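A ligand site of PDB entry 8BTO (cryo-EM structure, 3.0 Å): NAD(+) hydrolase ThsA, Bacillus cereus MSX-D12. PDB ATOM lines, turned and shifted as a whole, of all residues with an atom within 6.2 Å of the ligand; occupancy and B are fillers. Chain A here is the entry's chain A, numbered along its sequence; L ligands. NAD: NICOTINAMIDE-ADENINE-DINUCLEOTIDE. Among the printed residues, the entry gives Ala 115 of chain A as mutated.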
ATOM      1  N   GLY A  31      -9.868  -5.875  12.181  1.00  0.00           N
ATOM      2  CA  GLY A  31      -9.241  -5.527  10.921  1.00  0.00           C
ATOM      3  C   GLY A  31      -8.325  -4.330  11.060  1.00  0.00           C
ATOM      4  O   GLY A  31      -7.997  -3.876  12.166  1.00  0.00           O
ATOM      5  N   ALA A  32      -7.913  -3.802   9.912  1.00  0.00           N
ATOM      6  CA  ALA A  32      -7.034  -2.635   9.906  1.00  0.00           C
ATOM      7  C   ALA A  32      -7.757  -1.383  10.378  1.00  0.00           C
ATOM      8  O   ALA A  32      -7.108  -0.423  10.826  1.00  0.00           O
ATOM      9  CB  ALA A  32      -6.441  -2.420   8.522  1.00  0.00           C
ATOM     10  N   GLY A  33      -9.088  -1.357  10.278  1.00  0.00           N
ATOM     11  CA  GLY A  33      -9.822  -0.158  10.618  1.00  0.00           C
ATOM     12  C   GLY A  33      -9.811   0.165  12.101  1.00  0.00           C
ATOM     13  O   GLY A  33      -9.962   1.331  12.487  1.00  0.00           O
ATOM     14  N   LEU A  34      -9.635  -0.848  12.946  1.00  0.00           N
ATOM     15  CA  LEU A  34      -9.592  -0.601  14.383  1.00  0.00           C
ATOM     16  C   LEU A  34      -8.351   0.179  14.789  1.00  0.00           C
ATOM     17  O   LEU A  34      -8.367   0.828  15.839  1.00  0.00           O
ATOM     18  CB  LEU A  34      -9.654  -1.932  15.142  1.00  0.00           C
ATOM     19  CG  LEU A  34      -9.946  -1.845  16.641  1.00  0.00           C
ATOM     20  CD1 LEU A  34     -11.209  -1.034  16.881  1.00  0.00           C
ATOM     21  CD2 LEU A  34     -10.071  -3.226  17.253  1.00  0.00           C
ATOM     22  N   SER A  35      -7.287   0.126  13.984  1.00  0.00           N
ATOM     23  CA  SER A  35      -6.070   0.864  14.273  1.00  0.00           C
ATOM     24  C   SER A  35      -5.969   2.195  13.537  1.00  0.00           C
ATOM     25  O   SER A  35      -5.115   3.014  13.890  1.00  0.00           O
ATOM     26  CB  SER A  35      -4.844   0.014  13.924  1.00  0.00           C
ATOM     27  OG  SER A  35      -4.809  -0.267  12.537  1.00  0.00           O
ATOM     28  N   MET A  36      -6.820   2.423  12.531  1.00  0.00           N
ATOM     29  CA  MET A  36      -6.761   3.678  11.795  1.00  0.00           C
ATOM     30  C   MET A  36      -7.158   4.872  12.642  1.00  0.00           C
ATOM     31  O   MET A  36      -6.823   6.012  12.291  1.00  0.00           O
ATOM     32  CB  MET A  36      -7.638   3.600  10.548  1.00  0.00           C
ATOM     33  CG  MET A  36      -7.048   2.769   9.427  1.00  0.00           C
ATOM     34  SD  MET A  36      -8.156   2.614   8.011  1.00  0.00           S
ATOM     35  CE  MET A  36      -8.466   4.333   7.627  1.00  0.00           C
ATOM     36  N   SER A  37      -7.882   4.657  13.738  1.00  0.00           N
ATOM     37  CA  SER A  37      -8.193   5.736  14.666  1.00  0.00           C
ATOM     38  C   SER A  37      -7.005   6.088  15.559  1.00  0.00           C
ATOM     39  O   SER A  37      -7.001   7.170  16.150  1.00  0.00           O
ATOM     40  CB  SER A  37      -9.393   5.365  15.530  1.00  0.00           C
ATOM     41  OG  SER A  37      -9.135   4.201  16.296  1.00  0.00           O
ATOM     42  N   VAL A  38      -6.028   5.193  15.666  1.00  0.00           N
ATOM     43  CA  VAL A  38      -4.895   5.436  16.557  1.00  0.00           C
ATOM     44  C   VAL A  38      -4.007   6.550  16.010  1.00  0.00           C
ATOM     45  O   VAL A  38      -3.510   7.395  16.771  1.00  0.00           O
ATOM     46  CB  VAL A  38      -4.101   4.132  16.765  1.00  0.00           C
ATOM     47  CG1 VAL A  38      -2.898   4.386  17.652  1.00  0.00           C
ATOM     48  CG2 VAL A  38      -4.994   3.073  17.359  1.00  0.00           C
ATOM     49  N   SER A  42      -3.574   5.482   6.414  1.00  0.00           N
ATOM     50  CA  SER A  42      -4.253   4.397   5.730  1.00  0.00           C
ATOM     51  C   SER A  42      -3.302   3.707   4.744  1.00  0.00           C
ATOM     52  O   SER A  42      -2.329   4.290   4.270  1.00  0.00           O
ATOM     53  CB  SER A  42      -5.487   4.916   4.979  1.00  0.00           C
ATOM     54  OG  SER A  42      -6.133   3.871   4.270  1.00  0.00           O
ATOM     55  N   TRP A  43      -3.618   2.449   4.450  1.00  0.00           N
ATOM     56  CA  TRP A  43      -2.773   1.669   3.539  1.00  0.00           C
ATOM     57  C   TRP A  43      -2.725   2.303   2.151  1.00  0.00           C
ATOM     58  O   TRP A  43      -1.691   2.221   1.471  1.00  0.00           O
ATOM     59  CB  TRP A  43      -3.292   0.231   3.467  1.00  0.00           C
ATOM     60  CG  TRP A  43      -2.483  -0.662   2.590  1.00  0.00           C
ATOM     61  CD1 TRP A  43      -2.940  -1.445   1.572  1.00  0.00           C
ATOM     62  CD2 TRP A  43      -1.061  -0.882   2.651  1.00  0.00           C
ATOM     63  NE1 TRP A  43      -1.906  -2.140   0.999  1.00  0.00           N
ATOM     64  CE2 TRP A  43      -0.743  -1.801   1.642  1.00  0.00           C
ATOM     65  CE3 TRP A  43      -0.038  -0.383   3.456  1.00  0.00           C
ATOM     66  CZ2 TRP A  43       0.561  -2.237   1.415  1.00  0.00           C
ATOM     67  CZ3 TRP A  43       1.253  -0.808   3.230  1.00  0.00           C
ATOM     68  CH2 TRP A  43       1.540  -1.728   2.227  1.00  0.00           C
ATOM     69  N   ASN A  99     -10.654   1.714  22.587  1.00  0.00           N
ATOM     70  CA  ASN A  99     -11.182   0.425  22.171  1.00  0.00           C
ATOM     71  C   ASN A  99     -10.231  -0.710  22.530  1.00  0.00           C
ATOM     72  O   ASN A  99     -10.658  -1.756  23.005  1.00  0.00           O
ATOM     73  CB  ASN A  99     -11.471   0.435  20.680  1.00  0.00           C
ATOM     74  CG  ASN A  99     -12.271   1.641  20.245  1.00  0.00           C
ATOM     75  OD1 ASN A  99     -12.975   2.243  21.049  1.00  0.00           O
ATOM     76  ND2 ASN A  99     -12.152   2.001  18.976  1.00  0.00           N
ATOM     77  N   THR A 114      -5.913  -8.846  11.177  1.00  0.00           N
ATOM     78  CA  THR A 114      -5.297  -8.653   9.870  1.00  0.00           C
ATOM     79  C   THR A 114      -4.440  -7.394   9.835  1.00  0.00           C
ATOM     80  O   THR A 114      -4.063  -6.943   8.743  1.00  0.00           O
ATOM     81  CB  THR A 114      -6.361  -8.589   8.775  1.00  0.00           C
ATOM     82  OG1 THR A 114      -7.368  -7.628   9.140  1.00  0.00           O
ATOM     83  CG2 THR A 114      -7.009  -9.943   8.584  1.00  0.00           C
ATOM     84  N   ALA A 115      -4.134  -6.817  10.990  1.00  0.00           N
ATOM     85  CA  ALA A 115      -3.297  -5.630  11.091  1.00  0.00           C
ATOM     86  C   ALA A 115      -1.905  -6.019  11.558  1.00  0.00           C
ATOM     87  O   ALA A 115      -1.748  -6.878  12.427  1.00  0.00           O
ATOM     88  CB  ALA A 115      -3.915  -4.606  12.040  1.00  0.00           C
ATOM     89  N   VAL A 197     -14.830  -6.245  14.266  1.00  0.00           N
ATOM     90  CA  VAL A 197     -14.731  -4.804  14.495  1.00  0.00           C
ATOM     91  C   VAL A 197     -13.687  -4.240  13.532  1.00  0.00           C
ATOM     92  O   VAL A 197     -12.597  -4.793  13.404  1.00  0.00           O
ATOM     93  CB  VAL A 197     -14.389  -4.477  15.953  1.00  0.00           C
ATOM     94  CG1 VAL A 197     -15.594  -4.705  16.841  1.00  0.00           C
ATOM     95  CG2 VAL A 197     -13.222  -5.339  16.431  1.00  0.00           C
ATOM     96  N   GLY A 198     -14.036  -3.149  12.871  1.00  0.00           N
ATOM     97  CA  GLY A 198     -13.109  -2.500  11.967  1.00  0.00           C
ATOM     98  C   GLY A 198     -12.653  -3.362  10.811  1.00  0.00           C
ATOM     99  O   GLY A 198     -11.485  -3.296  10.415  1.00  0.00           O
ATOM    100  N   PHE A 199     -13.551  -4.173  10.265  1.00  0.00           N
ATOM    101  CA  PHE A 199     -13.225  -5.062   9.152  1.00  0.00           C
ATOM    102  C   PHE A 199     -14.166  -4.775   7.992  1.00  0.00           C
ATOM    103  O   PHE A 199     -15.359  -4.572   8.178  1.00  0.00           O
ATOM    104  CB  PHE A 199     -13.339  -6.532   9.574  1.00  0.00           C
ATOM    105  CG  PHE A 199     -12.737  -7.485   8.601  1.00  0.00           C
ATOM    106  CD1 PHE A 199     -11.424  -7.331   8.180  1.00  0.00           C
ATOM    107  CD2 PHE A 199     -13.474  -8.535   8.087  1.00  0.00           C
ATOM    108  CE1 PHE A 199     -10.865  -8.204   7.275  1.00  0.00           C
ATOM    109  CE2 PHE A 199     -12.914  -9.416   7.188  1.00  0.00           C
ATOM    110  CZ  PHE A 199     -11.616  -9.244   6.775  1.00  0.00           C
ATOM    111  N   SER A 200     -13.603  -4.761   6.785  1.00  0.00           N
ATOM    112  CA  SER A 200     -14.344  -4.399   5.586  1.00  0.00           C
ATOM    113  C   SER A 200     -14.910  -5.591   4.834  1.00  0.00           C
ATOM    114  O   SER A 200     -15.717  -5.394   3.920  1.00  0.00           O
ATOM    115  CB  SER A 200     -13.454  -3.590   4.642  1.00  0.00           C
ATOM    116  OG  SER A 200     -12.306  -4.326   4.269  1.00  0.00           O
ATOM    117  N   PHE A 201     -14.505  -6.810   5.191  1.00  0.00           N
ATOM    118  CA  PHE A 201     -14.986  -8.036   4.532  1.00  0.00           C
ATOM    119  C   PHE A 201     -14.709  -8.017   3.032  1.00  0.00           C
ATOM    120  O   PHE A 201     -15.503  -8.525   2.227  1.00  0.00           O
ATOM    121  CB  PHE A 201     -16.467  -8.274   4.807  1.00  0.00           C
ATOM    122  CG  PHE A 201     -16.759  -8.714   6.207  1.00  0.00           C
ATOM    123  CD1 PHE A 201     -16.736 -10.049   6.536  1.00  0.00           C
ATOM    124  CD2 PHE A 201     -17.046  -7.786   7.189  1.00  0.00           C
ATOM    125  CE1 PHE A 201     -16.989 -10.458   7.826  1.00  0.00           C
ATOM    126  CE2 PHE A 201     -17.310  -8.190   8.471  1.00  0.00           C
ATOM    127  CZ  PHE A 201     -17.285  -9.531   8.793  1.00  0.00           C
ATOM    128  N   THR A 202     -13.584  -7.437   2.641  1.00  0.00           N
ATOM    129  CA  THR A 202     -13.110  -7.494   1.270  1.00  0.00           C
ATOM    130  C   THR A 202     -11.832  -8.306   1.130  1.00  0.00           C
ATOM    131  O   THR A 202     -11.281  -8.397   0.036  1.00  0.00           O
ATOM    132  CB  THR A 202     -12.882  -6.083   0.713  1.00  0.00           C
ATOM    133  OG1 THR A 202     -11.891  -5.409   1.494  1.00  0.00           O
ATOM    134  CG2 THR A 202     -14.173  -5.282   0.738  1.00  0.00           C
ATOM    135  N   ASP A 203     -11.358  -8.903   2.219  1.00  0.00           N
ATOM    136  CA  ASP A 203     -10.111  -9.649   2.175  1.00  0.00           C
ATOM    137  C   ASP A 203     -10.325 -10.990   1.496  1.00  0.00           C
ATOM    138  O   ASP A 203     -11.232 -11.742   1.890  1.00  0.00           O
ATOM    139  CB  ASP A 203      -9.575  -9.854   3.590  1.00  0.00           C
ATOM    140  CG  ASP A 203      -8.139 -10.331   3.606  1.00  0.00           C
ATOM    141  OD1 ASP A 203      -7.252  -9.540   3.214  1.00  0.00           O
ATOM    142  OD2 ASP A 203      -7.897 -11.484   4.011  1.00  0.00           O
ATOM    143  N   LEU A 227     -19.619  -5.016  13.097  1.00  0.00           N
ATOM    144  CA  LEU A 227     -19.856  -3.591  13.306  1.00  0.00           C
ATOM    145  C   LEU A 227     -19.371  -2.836  12.075  1.00  0.00           C
ATOM    146  O   LEU A 227     -18.170  -2.841  11.775  1.00  0.00           O
ATOM    147  CB  LEU A 227     -19.145  -3.088  14.562  1.00  0.00           C
ATOM    148  CG  LEU A 227     -19.527  -3.736  15.888  1.00  0.00           C
ATOM    149  CD1 LEU A 227     -18.817  -3.044  17.051  1.00  0.00           C
ATOM    150  CD2 LEU A 227     -21.023  -3.688  16.090  1.00  0.00           C
ATOM    151  N   ILE A 228     -20.297  -2.200  11.371  1.00  0.00           N
ATOM    152  CA  ILE A 228     -19.999  -1.441  10.156  1.00  0.00           C
ATOM    153  C   ILE A 228     -20.695  -0.094  10.245  1.00  0.00           C
ATOM    154  O   ILE A 228     -21.874  -0.019  10.572  1.00  0.00           O
ATOM    155  CB  ILE A 228     -20.428  -2.210   8.891  1.00  0.00           C
ATOM    156  CG1 ILE A 228     -19.429  -3.314   8.567  1.00  0.00           C
ATOM    157  CG2 ILE A 228     -20.582  -1.259   7.716  1.00  0.00           C
ATOM    158  CD1 ILE A 228     -19.756  -4.080   7.313  1.00  0.00           C
ATOM    159  N   LYS A 229     -19.952   0.970   9.944  1.00  0.00           N
ATOM    160  CA  LYS A 229     -20.520   2.317   9.945  1.00  0.00           C
ATOM    161  C   LYS A 229     -21.366   2.531   8.698  1.00  0.00           C
ATOM    162  O   LYS A 229     -20.966   2.134   7.599  1.00  0.00           O
ATOM    163  CB  LYS A 229     -19.420   3.367  10.018  1.00  0.00           C
ATOM    164  CG  LYS A 229     -19.937   4.801  10.012  1.00  0.00           C
ATOM    165  CD  LYS A 229     -18.798   5.804   9.933  1.00  0.00           C
ATOM    166  CE  LYS A 229     -18.070   5.713   8.604  1.00  0.00           C
ATOM    167  NZ  LYS A 229     -18.966   6.025   7.461  1.00  0.00           N
ATOM    168  N   TYR A 269     -18.171   6.303  14.122  1.00  0.00           N
ATOM    169  CA  TYR A 269     -17.084   5.437  14.568  1.00  0.00           C
ATOM    170  C   TYR A 269     -16.977   5.447  16.090  1.00  0.00           C
ATOM    171  O   TYR A 269     -16.625   4.433  16.700  1.00  0.00           O
ATOM    172  CB  TYR A 269     -15.760   5.884  13.941  1.00  0.00           C
ATOM    173  CG  TYR A 269     -15.577   5.385  12.523  1.00  0.00           C
ATOM    174  CD1 TYR A 269     -16.092   4.165  12.119  1.00  0.00           C
ATOM    175  CD2 TYR A 269     -14.879   6.132  11.597  1.00  0.00           C
ATOM    176  CE1 TYR A 269     -15.914   3.701  10.831  1.00  0.00           C
ATOM    177  CE2 TYR A 269     -14.696   5.692  10.304  1.00  0.00           C
ATOM    178  CZ  TYR A 269     -15.212   4.469   9.928  1.00  0.00           C
ATOM    179  OH  TYR A 269     -15.038   4.020   8.641  1.00  0.00           O
ATOM    180  N   ILE A 272     -18.571   2.765  18.451  1.00  0.00           N
ATOM    181  CA  ILE A 272     -17.916   1.499  18.792  1.00  0.00           C
ATOM    182  C   ILE A 272     -17.440   1.532  20.242  1.00  0.00           C
ATOM    183  O   ILE A 272     -17.622   0.566  20.993  1.00  0.00           O
ATOM    184  CB  ILE A 272     -16.742   1.235  17.834  1.00  0.00           C
ATOM    185  CG1 ILE A 272     -17.225   1.230  16.386  1.00  0.00           C
ATOM    186  CG2 ILE A 272     -16.083  -0.087  18.157  1.00  0.00           C
ATOM    187  CD1 ILE A 272     -16.145   0.901  15.378  1.00  0.00           C
HETATM  188  PA  NAD L   1      -9.611  -1.373   5.757  1.00  0.00           P
HETATM  189  O1A NAD L   1     -10.255  -1.710   4.429  1.00  0.00           O
HETATM  190  O2A NAD L   1      -8.767  -0.134   5.883  1.00  0.00           O
HETATM  191  O5B NAD L   1     -10.760  -1.286   6.873  1.00  0.00           O
HETATM  192  C5B NAD L   1     -11.977  -0.594   6.581  1.00  0.00           C
HETATM  193  C4B NAD L   1     -13.014  -0.914   7.645  1.00  0.00           C
HETATM  194  O4B NAD L   1     -12.566  -0.388   8.894  1.00  0.00           O
HETATM  195  C3B NAD L   1     -14.360  -0.281   7.331  1.00  0.00           C
HETATM  196  O3B NAD L   1     -15.395  -1.254   7.465  1.00  0.00           O
HETATM  197  C2B NAD L   1     -14.536   0.818   8.357  1.00  0.00           C
HETATM  198  O2B NAD L   1     -15.849   0.758   8.926  1.00  0.00           O
HETATM  199  C1B NAD L   1     -13.494   0.554   9.430  1.00  0.00           C
HETATM  200  N9A NAD L   1     -12.766   1.802   9.773  1.00  0.00           N
HETATM  201  C8A NAD L   1     -12.090   2.582   8.919  1.00  0.00           C
HETATM  202  N7A NAD L   1     -11.538   3.646   9.548  1.00  0.00           N
HETATM  203  C5A NAD L   1     -11.857   3.548  10.850  1.00  0.00           C
HETATM  204  C6A NAD L   1     -11.586   4.339  12.068  1.00  0.00           C
HETATM  205  N6A NAD L   1     -10.850   5.466  12.020  1.00  0.00           N
HETATM  206  N1A NAD L   1     -12.103   3.893  13.241  1.00  0.00           N
HETATM  207  C2A NAD L   1     -12.839   2.765  13.303  1.00  0.00           C
HETATM  208  N3A NAD L   1     -13.121   1.992  12.227  1.00  0.00           N
HETATM  209  C4A NAD L   1     -12.669   2.330  10.996  1.00  0.00           C
HETATM  210  O3  NAD L   1      -8.707  -2.628   6.220  1.00  0.00           O
HETATM  211  PN  NAD L   1      -9.208  -4.151   6.186  1.00  0.00           P
HETATM  212  O1N NAD L   1     -10.671  -4.187   6.560  1.00  0.00           O
HETATM  213  O2N NAD L   1      -8.225  -4.997   6.963  1.00  0.00           O
HETATM  214  O5D NAD L   1      -9.083  -4.554   4.631  1.00  0.00           O
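The side-chain hydroxyl of Ser 200 sits at hydrogen-bond distance from the side-chain hydroxyl of Thr 202 (3.0 Å). O of Ala 32 sits at hydrogen-bond distance from OG of Ser 35, at 2.9 Å. N of Gly 33 is in hydrogen-bond range of O of Gly 198. OG of Ser 37 lies within hydrogen-bond range of O of Leu 34, 3.5 Å away.
The backbone NH of Ser 200 sits at hydrogen-bond distance from an oxygen (O1N) of the ligand (3.0 Å). OG of Ser 200 is in hydrogen-bond range of O1N of the ligand. N of Ala 32 lies within hydrogen-bond range of O2N of the ligand, 3.2 Å away. The side-chain hydroxyl (OH) of Tyr 269 sits close to an oxygen (O2B) of the ligand (3.4 Å). O of Phe 199 is in hydrogen-bond range of O3B of the ligand.
The backbone carbonyl oxygen (O) of Gly 33 lies close to a nitrogen (N3A) of the ligand, 3.2 Å away. SD of Met 36 lies close to O2A of the ligand (3.5 Å). An oxygen (O4B) of the ligand sits close to the backbone carbonyl oxygen of Gly 198 (3.5 Å). Residues that only touch the ligand: Thr 114 (3.5 Å) and Ser 37 (3.5 Å). Hydrophobic or aromatic side chains that line the ligand: Ala 32, Met 36, Phe 199 and Tyr 269.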
